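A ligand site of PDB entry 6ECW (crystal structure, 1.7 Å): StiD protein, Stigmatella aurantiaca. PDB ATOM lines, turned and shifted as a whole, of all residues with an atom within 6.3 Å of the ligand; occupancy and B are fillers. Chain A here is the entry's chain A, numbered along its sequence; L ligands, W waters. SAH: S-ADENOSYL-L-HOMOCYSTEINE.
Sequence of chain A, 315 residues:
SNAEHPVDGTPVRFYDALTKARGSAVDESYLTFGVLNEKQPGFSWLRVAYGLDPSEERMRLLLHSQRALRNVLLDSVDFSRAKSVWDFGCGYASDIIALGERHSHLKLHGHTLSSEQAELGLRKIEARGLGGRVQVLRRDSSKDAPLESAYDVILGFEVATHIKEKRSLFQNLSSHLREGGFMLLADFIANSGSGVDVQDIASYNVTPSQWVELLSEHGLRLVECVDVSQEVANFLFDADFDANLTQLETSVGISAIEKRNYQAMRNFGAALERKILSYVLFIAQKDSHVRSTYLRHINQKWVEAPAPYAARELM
O3' of the ligand is in hydrogen-bond range of OE1 of Gln 117 (2.7 Å). N of Ser 141 is in hydrogen-bond range of N1 of the ligand. O2' of the ligand is in hydrogen-bond range of OG1 of Thr 112, 2.8 Å away. N6 of the ligand lies within hydrogen-bond range of OD1 of Asp 140, 2.9 Å away. OXT of the ligand lies within salt-bridge range of NH2 of Arg 70. The backbone carbonyl oxygen (O) of Phe 157 lies within hydrogen-bond range of a nitrogen (N) of the ligand, at 3.0 Å. O3' of the ligand lies within hydrogen-bond range of N of Gly 91 (3.1 Å). An oxygen (O2') of the ligand sits at hydrogen-bond distance from the backbone NH (N) of Leu 113, 3.3 Å away. O of Gly 89 is in hydrogen-bond range of N of the ligand, 3.4 Å away.
OE1 of Gln 117 lies within hydrogen-bond range of OG1 of Thr 112, at 2.7 Å. The side-chain amide oxygen (OE1) of Gln 117 lies close to the backbone carbonyl oxygen (O) of Gly 91. OG of Ser 141 sits at hydrogen-bond distance from O of Phe 88, at 2.8 Å. The side-chain hydroxyl of Ser 141 is in hydrogen-bond range of a ring nitrogen (ND1) of His 111, at 3.1 Å. The backbone carbonyl oxygen (O) of Thr 112 sits at hydrogen-bond distance from the backbone NH (N) of Arg 139 (3.3 Å). OG of Ser 142 sits at hydrogen-bond distance from OD1 of Asp 140 (2.5 Å). The side-chain hydroxyl (OG1) of Thr 32 is in hydrogen-bond range of the backbone carbonyl oxygen (O) of Ser 29 (2.9 Å). The backbone carbonyl oxygen (O) of His 111 is in hydrogen-bond range of the backbone NH (N) of Cys 90, 2.8 Å away.
O of Phe 88 sits close to N3 of the ligand. O of Glu 158 sits close to SD of the ligand. Glu 28 touches the ligand. CG2 of Thr 32 touches OXT of the ligand, at 3.6 Å. Asp 95 touches the ligand. His 111 touches the ligand. O of Arg 139 touches C2 of the ligand (3.2 Å). CG1 of Val 159 touches O4' of the ligand, at 3.9 Å. His 162 touches the ligand. Ile 163 touches the ligand. Hydrophobic or aromatic side chains within 4 Å of the ligand: Leu 113, Phe 157, Val 159, His 162 and Ile 163. Within 4 Å of the ligand: Glu 28, Thr 32, Arg 70, Phe 88, Gly 89, Gly 91, Asp 95, His 111, Thr 112, Leu 113, Gln 117, Arg 139, Asp 140, Ser 141, Phe 157, Glu 158, Val 159, His 162 and Ile 163. The nearest printed residue that does not touch the ligand is Cys 90 (4.1 Å).
Water W4 bridges O of His 162 (2.7 Å) and N7 of the ligand (2.7 Å). Water W2 lies within hydrogen-bond range of an oxygen (O) of the ligand, the side-chain hydroxyl (OG) of Ser 94 and the backbone NH (N) of Tyr 92. Water W5 lies within hydrogen-bond range of OD2 of Asp 87 (2.6 Å), OD2 of Asp 95 (2.6 Å) and N of the ligand (3.2 Å). Water W3 lies within hydrogen-bond range of OD1 of Asp 87 (2.7 Å), N of Phe 157 (2.8 Å), O of Gly 89 (3.1 Å) and N of the ligand (3.4 Å).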
ATOM      1  N   GLU A  28      -3.579  32.392   0.104  1.00  0.00           N
ATOM      2  CA  GLU A  28      -2.225  31.931   0.427  1.00  0.00           C
ATOM      3  C   GLU A  28      -2.058  30.444   0.142  1.00  0.00           C
ATOM      4  O   GLU A  28      -0.946  30.004  -0.206  1.00  0.00           O
ATOM      5  CB  GLU A  28      -1.908  32.248   1.890  1.00  0.00           C
ATOM      6  CG  GLU A  28      -0.617  31.595   2.422  1.00  0.00           C
ATOM      7  CD  GLU A  28       0.585  31.786   1.509  1.00  0.00           C
ATOM      8  OE1 GLU A  28       0.754  32.900   0.951  1.00  0.00           O
ATOM      9  OE2 GLU A  28       1.360  30.810   1.326  1.00  0.00           O
ATOM     10  N   SER A  29      -3.131  29.644   0.261  1.00  0.00           N
ATOM     11  CA  SER A  29      -3.024  28.232  -0.082  1.00  0.00           C
ATOM     12  C   SER A  29      -2.525  28.032  -1.519  1.00  0.00           C
ATOM     13  O   SER A  29      -1.790  27.075  -1.791  1.00  0.00           O
ATOM     14  CB  SER A  29      -4.365  27.506   0.146  1.00  0.00           C
ATOM     15  OG  SER A  29      -5.410  28.086  -0.617  1.00  0.00           O
ATOM     16  N   THR A  32       1.546  27.913  -1.654  1.00  0.00           N
ATOM     17  CA  THR A  32       2.320  26.930  -0.888  1.00  0.00           C
ATOM     18  C   THR A  32       3.021  25.950  -1.827  1.00  0.00           C
ATOM     19  O   THR A  32       2.759  25.903  -3.037  1.00  0.00           O
ATOM     20  CB  THR A  32       1.418  26.160   0.078  1.00  0.00           C
ATOM     21  OG1 THR A  32       0.376  25.515  -0.674  1.00  0.00           O
ATOM     22  CG2 THR A  32       0.765  27.069   1.089  1.00  0.00           C
ATOM     23  N   ARG A  70      -0.212  18.291   1.432  1.00  0.00           N
ATOM     24  CA  ARG A  70      -0.841  18.409   2.732  1.00  0.00           C
ATOM     25  C   ARG A  70      -1.425  17.074   3.164  1.00  0.00           C
ATOM     26  O   ARG A  70      -1.375  16.732   4.351  1.00  0.00           O
ATOM     27  CB  ARG A  70      -1.931  19.480   2.697  1.00  0.00           C
ATOM     28  CG  ARG A  70      -1.526  20.734   3.468  1.00  0.00           C
ATOM     29  CD  ARG A  70      -1.209  21.901   2.552  1.00  0.00           C
ATOM     30  NE  ARG A  70      -0.970  23.123   3.310  1.00  0.00           N
ATOM     31  CZ  ARG A  70       0.212  23.748   3.409  1.00  0.00           C
ATOM     32  NH1 ARG A  70       1.285  23.253   2.777  1.00  0.00           N
ATOM     33  NH2 ARG A  70       0.316  24.859   4.139  1.00  0.00           N
ATOM     34  N   ASP A  87      -2.324  25.005  15.036  1.00  0.00           N
ATOM     35  CA  ASP A  87      -1.403  25.348  13.938  1.00  0.00           C
ATOM     36  C   ASP A  87      -0.461  26.431  14.472  1.00  0.00           C
ATOM     37  O   ASP A  87      -0.895  27.576  14.678  1.00  0.00           O
ATOM     38  CB  ASP A  87      -2.190  25.803  12.711  1.00  0.00           C
ATOM     39  CG  ASP A  87      -1.285  26.100  11.525  1.00  0.00           C
ATOM     40  OD1 ASP A  87      -0.085  26.335  11.752  1.00  0.00           O
ATOM     41  OD2 ASP A  87      -1.783  26.174  10.383  1.00  0.00           O
ATOM     42  N   PHE A  88       0.808  26.091  14.717  1.00  0.00           N
ATOM     43  CA  PHE A  88       1.656  27.027  15.461  1.00  0.00           C
ATOM     44  C   PHE A  88       2.336  28.063  14.590  1.00  0.00           C
ATOM     45  O   PHE A  88       3.049  28.909  15.130  1.00  0.00           O
ATOM     46  CB  PHE A  88       2.689  26.284  16.358  1.00  0.00           C
ATOM     47  CG  PHE A  88       3.754  25.482  15.638  1.00  0.00           C
ATOM     48  CD1 PHE A  88       5.002  26.052  15.338  1.00  0.00           C
ATOM     49  CD2 PHE A  88       3.542  24.141  15.354  1.00  0.00           C
ATOM     50  CE1 PHE A  88       5.992  25.272  14.709  1.00  0.00           C
ATOM     51  CE2 PHE A  88       4.525  23.374  14.742  1.00  0.00           C
ATOM     52  CZ  PHE A  88       5.778  23.960  14.402  1.00  0.00           C
ATOM     53  N   GLY A  89       2.060  28.077  13.298  1.00  0.00           N
ATOM     54  CA  GLY A  89       2.435  29.234  12.481  1.00  0.00           C
ATOM     55  C   GLY A  89       1.488  29.265  11.296  1.00  0.00           C
ATOM     56  O   GLY A  89       1.807  28.725  10.234  1.00  0.00           O
ATOM     57  N   CYS A  90       0.309  29.868  11.475  1.00  0.00           N
ATOM     58  CA  CYS A  90      -0.829  29.524  10.630  1.00  0.00           C
ATOM     59  C   CYS A  90      -0.964  30.398   9.386  1.00  0.00           C
ATOM     60  O   CYS A  90      -1.941  30.242   8.655  1.00  0.00           O
ATOM     61  CB  CYS A  90      -2.120  29.569  11.450  1.00  0.00           C
ATOM     62  SG  CYS A  90      -2.495  31.213  12.098  1.00  0.00           S
ATOM     63  N   GLY A  91      -0.022  31.304   9.109  1.00  0.00           N
ATOM     64  CA  GLY A  91      -0.181  32.220   7.989  1.00  0.00           C
ATOM     65  C   GLY A  91      -1.515  32.952   8.034  1.00  0.00           C
ATOM     66  O   GLY A  91      -1.892  33.538   9.062  1.00  0.00           O
ATOM     67  N   TYR A  92      -2.257  32.893   6.917  1.00  0.00           N
ATOM     68  CA  TYR A  92      -3.603  33.450   6.829  1.00  0.00           C
ATOM     69  C   TYR A  92      -4.693  32.447   7.182  1.00  0.00           C
ATOM     70  O   TYR A  92      -5.847  32.616   6.781  1.00  0.00           O
ATOM     71  CB  TYR A  92      -3.833  34.040   5.423  1.00  0.00           C
ATOM     72  CG  TYR A  92      -2.963  35.241   5.138  1.00  0.00           C
ATOM     73  CD1 TYR A  92      -3.308  36.498   5.595  1.00  0.00           C
ATOM     74  CD2 TYR A  92      -1.774  35.113   4.409  1.00  0.00           C
ATOM     75  CE1 TYR A  92      -2.510  37.608   5.336  1.00  0.00           C
ATOM     76  CE2 TYR A  92      -0.958  36.224   4.150  1.00  0.00           C
ATOM     77  CZ  TYR A  92      -1.326  37.459   4.611  1.00  0.00           C
ATOM     78  OH  TYR A  92      -0.534  38.558   4.363  1.00  0.00           O
ATOM     79  N   ALA A  93      -4.337  31.384   7.927  1.00  0.00           N
ATOM     80  CA  ALA A  93      -5.274  30.436   8.535  1.00  0.00           C
ATOM     81  C   ALA A  93      -6.014  29.564   7.516  1.00  0.00           C
ATOM     82  O   ALA A  93      -7.012  28.940   7.855  1.00  0.00           O
ATOM     83  CB  ALA A  93      -6.290  31.146   9.439  1.00  0.00           C
ATOM     84  N   SER A  94      -5.513  29.471   6.279  1.00  0.00           N
ATOM     85  CA  SER A  94      -6.161  28.634   5.265  1.00  0.00           C
ATOM     86  C   SER A  94      -6.296  27.176   5.714  1.00  0.00           C
ATOM     87  O   SER A  94      -7.339  26.542   5.490  1.00  0.00           O
ATOM     88  CB  SER A  94      -5.371  28.700   3.964  1.00  0.00           C
ATOM     89  OG  SER A  94      -5.531  29.977   3.388  1.00  0.00           O
ATOM     90  N   ASP A  95      -5.240  26.624   6.295  1.00  0.00           N
ATOM     91  CA  ASP A  95      -5.249  25.223   6.704  1.00  0.00           C
ATOM     92  C   ASP A  95      -6.282  24.954   7.809  1.00  0.00           C
ATOM     93  O   ASP A  95      -7.032  23.971   7.740  1.00  0.00           O
ATOM     94  CB  ASP A  95      -3.862  24.801   7.157  1.00  0.00           C
ATOM     95  CG  ASP A  95      -2.920  24.620   5.973  1.00  0.00           C
ATOM     96  OD1 ASP A  95      -3.383  24.142   4.919  1.00  0.00           O
ATOM     97  OD2 ASP A  95      -1.730  24.988   6.110  1.00  0.00           O
ATOM     98  N   HIS A 111      -1.472  30.321  15.515  1.00  0.00           N
ATOM     99  CA  HIS A 111      -0.586  31.365  16.005  1.00  0.00           C
ATOM    100  C   HIS A 111       0.129  32.019  14.831  1.00  0.00           C
ATOM    101  O   HIS A 111       0.556  31.323  13.890  1.00  0.00           O
ATOM    102  CB  HIS A 111       0.470  30.803  16.965  1.00  0.00           C
ATOM    103  CG  HIS A 111      -0.059  30.478  18.317  1.00  0.00           C
ATOM    104  ND1 HIS A 111       0.775  30.179  19.386  1.00  0.00           N
ATOM    105  CD2 HIS A 111      -1.323  30.421  18.801  1.00  0.00           C
ATOM    106  CE1 HIS A 111       0.035  29.962  20.464  1.00  0.00           C
ATOM    107  NE2 HIS A 111      -1.233  30.086  20.134  1.00  0.00           N
ATOM    108  N   THR A 112       0.307  33.338  14.902  1.00  0.00           N
ATOM    109  CA  THR A 112       1.043  34.060  13.878  1.00  0.00           C
ATOM    110  C   THR A 112       1.740  35.237  14.531  1.00  0.00           C
ATOM    111  O   THR A 112       1.271  35.777  15.544  1.00  0.00           O
ATOM    112  CB  THR A 112       0.135  34.530  12.748  1.00  0.00           C
ATOM    113  OG1 THR A 112       0.930  35.203  11.771  1.00  0.00           O
ATOM    114  CG2 THR A 112      -0.935  35.482  13.273  1.00  0.00           C
ATOM    115  N   LEU A 113       2.878  35.614  13.964  1.00  0.00           N
ATOM    116  CA  LEU A 113       3.622  36.758  14.496  1.00  0.00           C
ATOM    117  C   LEU A 113       3.131  38.092  13.962  1.00  0.00           C
ATOM    118  O   LEU A 113       3.433  39.132  14.555  1.00  0.00           O
ATOM    119  CB  LEU A 113       5.112  36.608  14.173  1.00  0.00           C
ATOM    120  CG  LEU A 113       5.905  35.582  14.966  1.00  0.00           C
ATOM    121  CD1 LEU A 113       7.318  35.492  14.410  1.00  0.00           C
ATOM    122  CD2 LEU A 113       5.903  35.967  16.436  1.00  0.00           C
ATOM    123  N   SER A 114       2.376  38.100  12.865  1.00  0.00           N
ATOM    124  CA  SER A 114       2.003  39.352  12.213  1.00  0.00           C
ATOM    125  C   SER A 114       0.558  39.730  12.523  1.00  0.00           C
ATOM    126  O   SER A 114      -0.334  38.879  12.523  1.00  0.00           O
ATOM    127  CB  SER A 114       2.163  39.285  10.695  1.00  0.00           C
ATOM    128  OG  SER A 114       1.257  38.337  10.158  1.00  0.00           O
ATOM    129  N   GLN A 117      -1.721  39.220   9.124  1.00  0.00           N
ATOM    130  CA  GLN A 117      -2.251  37.866   8.940  1.00  0.00           C
ATOM    131  C   GLN A 117      -3.346  37.575   9.941  1.00  0.00           C
ATOM    132  O   GLN A 117      -4.355  36.952   9.596  1.00  0.00           O
ATOM    133  CB  GLN A 117      -1.144  36.818   9.059  1.00  0.00           C
ATOM    134  CG  GLN A 117      -0.307  36.673   7.796  1.00  0.00           C
ATOM    135  CD  GLN A 117       0.931  35.862   8.002  1.00  0.00           C
ATOM    136  OE1 GLN A 117       1.111  35.229   9.033  1.00  0.00           O
ATOM    137  NE2 GLN A 117       1.827  35.893   7.025  1.00  0.00           N
ATOM    138  N   ARG A 139       0.704  35.304  18.796  1.00  0.00           N
ATOM    139  CA  ARG A 139       1.484  34.691  19.849  1.00  0.00           C
ATOM    140  C   ARG A 139       2.729  34.078  19.229  1.00  0.00           C
ATOM    141  O   ARG A 139       2.705  33.587  18.099  1.00  0.00           O
ATOM    142  CB  ARG A 139       0.691  33.597  20.587  1.00  0.00           C
ATOM    143  CG  ARG A 139      -0.368  34.184  21.524  1.00  0.00           C
ATOM    144  CD  ARG A 139      -1.121  33.095  22.292  1.00  0.00           C
ATOM    145  NE  ARG A 139      -2.146  33.727  23.123  1.00  0.00           N
ATOM    146  CZ  ARG A 139      -2.817  33.138  24.115  1.00  0.00           C
ATOM    147  NH1 ARG A 139      -2.582  31.873  24.419  1.00  0.00           N
ATOM    148  NH2 ARG A 139      -3.734  33.814  24.781  1.00  0.00           N
ATOM    149  N   ASP A 140       3.834  34.169  19.976  1.00  0.00           N
ATOM    150  CA  ASP A 140       5.139  33.645  19.582  1.00  0.00           C
ATOM    151  C   ASP A 140       5.217  32.212  20.107  1.00  0.00           C
ATOM    152  O   ASP A 140       5.425  31.982  21.300  1.00  0.00           O
ATOM    153  CB  ASP A 140       6.243  34.527  20.148  1.00  0.00           C
ATOM    154  CG  ASP A 140       7.621  34.056  19.792  1.00  0.00           C
ATOM    155  OD1 ASP A 140       7.795  32.929  19.252  1.00  0.00           O
ATOM    156  OD2 ASP A 140       8.568  34.823  20.043  1.00  0.00           O
ATOM    157  N   SER A 141       5.023  31.229  19.214  1.00  0.00           N
ATOM    158  CA  SER A 141       4.938  29.839  19.640  1.00  0.00           C
ATOM    159  C   SER A 141       6.230  29.305  20.252  1.00  0.00           C
ATOM    160  O   SER A 141       6.216  28.236  20.861  1.00  0.00           O
ATOM    161  CB  SER A 141       4.540  28.938  18.462  1.00  0.00           C
ATOM    162  OG  SER A 141       3.382  29.436  17.821  1.00  0.00           O
ATOM    163  N   SER A 142       7.353  30.005  20.100  1.00  0.00           N
ATOM    164  CA  SER A 142       8.562  29.540  20.768  1.00  0.00           C
ATOM    165  C   SER A 142       8.550  29.852  22.268  1.00  0.00           C
ATOM    166  O   SER A 142       9.353  29.282  23.012  1.00  0.00           O
ATOM    167  CB  SER A 142       9.797  30.161  20.118  1.00  0.00           C
ATOM    168  OG  SER A 142       9.759  31.593  20.168  1.00  0.00           O
ATOM    169  N   GLY A 156       2.591  22.136  11.765  1.00  0.00           N
ATOM    170  CA  GLY A 156       3.612  23.125  11.481  1.00  0.00           C
ATOM    171  C   GLY A 156       4.145  22.957  10.072  1.00  0.00           C
ATOM    172  O   GLY A 156       5.048  22.156   9.864  1.00  0.00           O
ATOM    173  N   PHE A 157       3.575  23.669   9.109  1.00  0.00           N
ATOM    174  CA  PHE A 157       4.013  23.576   7.707  1.00  0.00           C
ATOM    175  C   PHE A 157       5.013  24.695   7.455  1.00  0.00           C
ATOM    176  O   PHE A 157       4.641  25.884   7.396  1.00  0.00           O
ATOM    177  CB  PHE A 157       2.823  23.626   6.772  1.00  0.00           C
ATOM    178  CG  PHE A 157       1.780  22.587   7.082  1.00  0.00           C
ATOM    179  CD1 PHE A 157       2.121  21.424   7.758  1.00  0.00           C
ATOM    180  CD2 PHE A 157       0.464  22.768   6.748  1.00  0.00           C
ATOM    181  CE1 PHE A 157       1.179  20.489   8.059  1.00  0.00           C
ATOM    182  CE2 PHE A 157      -0.483  21.811   7.052  1.00  0.00           C
ATOM    183  CZ  PHE A 157      -0.138  20.689   7.693  1.00  0.00           C
ATOM    184  N   GLU A 158       6.290  24.317   7.355  1.00  0.00           N
ATOM    185  CA  GLU A 158       7.400  25.233   7.136  1.00  0.00           C
ATOM    186  C   GLU A 158       7.403  26.395   8.150  1.00  0.00           C
ATOM    187  O   GLU A 158       7.523  27.575   7.806  1.00  0.00           O
ATOM    188  CB  GLU A 158       7.391  25.752   5.702  1.00  0.00           C
ATOM    189  CG  GLU A 158       8.754  26.160   5.205  1.00  0.00           C
ATOM    190  CD  GLU A 158       8.652  27.070   3.975  1.00  0.00           C
ATOM    191  OE1 GLU A 158       7.671  26.902   3.192  1.00  0.00           O
ATOM    192  OE2 GLU A 158       9.521  27.955   3.817  1.00  0.00           O
ATOM    193  N   VAL A 159       7.250  26.050   9.431  1.00  0.00           N
ATOM    194  CA  VAL A 159       7.289  27.015  10.523  1.00  0.00           C
ATOM    195  C   VAL A 159       8.579  26.900  11.308  1.00  0.00           C
ATOM    196  O   VAL A 159       9.258  27.911  11.548  1.00  0.00           O
ATOM    197  CB  VAL A 159       6.074  26.840  11.459  1.00  0.00           C
ATOM    198  CG1 VAL A 159       6.155  27.937  12.540  1.00  0.00           C
ATOM    199  CG2 VAL A 159       4.768  26.884  10.711  1.00  0.00           C
ATOM    200  N   HIS A 162      11.733  28.625  10.565  1.00  0.00           N
ATOM    201  CA  HIS A 162      11.694  30.089  10.643  1.00  0.00           C
ATOM    202  C   HIS A 162      11.827  30.571  12.081  1.00  0.00           C
ATOM    203  O   HIS A 162      11.738  31.769  12.324  1.00  0.00           O
ATOM    204  CB  HIS A 162      10.401  30.624  10.031  1.00  0.00           C
ATOM    205  CG  HIS A 162      10.288  30.415   8.559  1.00  0.00           C
ATOM    206  ND1 HIS A 162      11.378  30.124   7.757  1.00  0.00           N
ATOM    207  CD2 HIS A 162       9.214  30.453   7.729  1.00  0.00           C
ATOM    208  CE1 HIS A 162      10.974  29.984   6.508  1.00  0.00           C
ATOM    209  NE2 HIS A 162       9.668  30.177   6.465  1.00  0.00           N
ATOM    210  N   ILE A 163      12.056  29.665  13.029  1.00  0.00           N
ATOM    211  CA  ILE A 163      12.091  29.986  14.444  1.00  0.00           C
ATOM    212  C   ILE A 163      13.502  29.712  14.932  1.00  0.00           C
ATOM    213  O   ILE A 163      14.010  28.602  14.797  1.00  0.00           O
ATOM    214  CB  ILE A 163      11.041  29.171  15.208  1.00  0.00           C
ATOM    215  CG1 ILE A 163       9.629  29.627  14.790  1.00  0.00           C
ATOM    216  CG2 ILE A 163      11.260  29.289  16.712  1.00  0.00           C
ATOM    217  CD1 ILE A 163       8.510  28.992  15.624  1.00  0.00           C
ATOM    218  N   LEU A 169      10.849  26.149  21.391  1.00  0.00           N
ATOM    219  CA  LEU A 169       9.676  25.810  20.583  1.00  0.00           C
ATOM    220  C   LEU A 169       9.229  24.387  20.860  1.00  0.00           C
ATOM    221  O   LEU A 169       8.058  24.138  21.192  1.00  0.00           O
ATOM    222  CB  LEU A 169       9.979  25.986  19.082  1.00  0.00           C
ATOM    223  CG  LEU A 169       8.898  25.472  18.089  1.00  0.00           C
ATOM    224  CD1 LEU A 169       7.635  26.351  18.140  1.00  0.00           C
ATOM    225  CD2 LEU A 169       9.416  25.420  16.644  1.00  0.00           C
HETATM  226  N   SAH L   1       2.148  27.518   7.058  1.00  0.00           N
HETATM  227  CA  SAH L   1       1.612  28.814   6.631  1.00  0.00           C
HETATM  228  CB  SAH L   1       2.760  29.801   6.548  1.00  0.00           C
HETATM  229  CG  SAH L   1       4.070  29.256   7.086  1.00  0.00           C
HETATM  230  SD  SAH L   1       5.426  30.442   6.888  1.00  0.00           S
HETATM  231  C   SAH L   1       0.817  28.793   5.306  1.00  0.00           C
HETATM  232  O   SAH L   1       0.243  29.815   4.914  1.00  0.00           O
HETATM  233  OXT SAH L   1       0.705  27.780   4.602  1.00  0.00           O
HETATM  234  C5' SAH L   1       5.598  30.773   8.664  1.00  0.00           C
HETATM  235  C4' SAH L   1       4.334  31.270   9.384  1.00  0.00           C
HETATM  236  O4' SAH L   1       4.554  31.025  10.747  1.00  0.00           O
HETATM  237  C3' SAH L   1       4.017  32.774   9.277  1.00  0.00           C
HETATM  238  O3' SAH L   1       2.624  32.977   9.164  1.00  0.00           O
HETATM  239  C2' SAH L   1       4.418  33.379  10.593  1.00  0.00           C
HETATM  240  O2' SAH L   1       3.526  34.389  11.013  1.00  0.00           O
HETATM  241  C1' SAH L   1       4.373  32.183  11.531  1.00  0.00           C
HETATM  242  N9  SAH L   1       5.486  32.195  12.478  1.00  0.00           N
HETATM  243  C8  SAH L   1       6.830  32.289  12.224  1.00  0.00           C
HETATM  244  N7  SAH L   1       7.488  32.257  13.409  1.00  0.00           N
HETATM  245  C5  SAH L   1       6.584  32.129  14.411  1.00  0.00           C
HETATM  246  C6  SAH L   1       6.676  32.062  15.802  1.00  0.00           C
HETATM  247  N6  SAH L   1       7.836  32.082  16.470  1.00  0.00           N
HETATM  248  N1  SAH L   1       5.524  31.931  16.538  1.00  0.00           N
HETATM  249  C2  SAH L   1       4.301  31.919  15.923  1.00  0.00           C
HETATM  250  N3  SAH L   1       4.185  31.999  14.549  1.00  0.00           N
HETATM  251  C4  SAH L   1       5.320  32.103  13.822  1.00  0.00           C
HETATM  252  O   HOH W   1      10.153  33.578  15.852  1.00  0.00           O
HETATM  253  O   HOH W   2      -2.717  30.657   4.685  1.00  0.00           O
HETATM  254  O   HOH W   3       1.706  25.652   9.806  1.00  0.00           O
HETATM  255  O   HOH W   4       9.921  33.517  13.178  1.00  0.00           O
HETATM  256  O   HOH W   5      -0.633  26.241   8.108  1.00  0.00           O
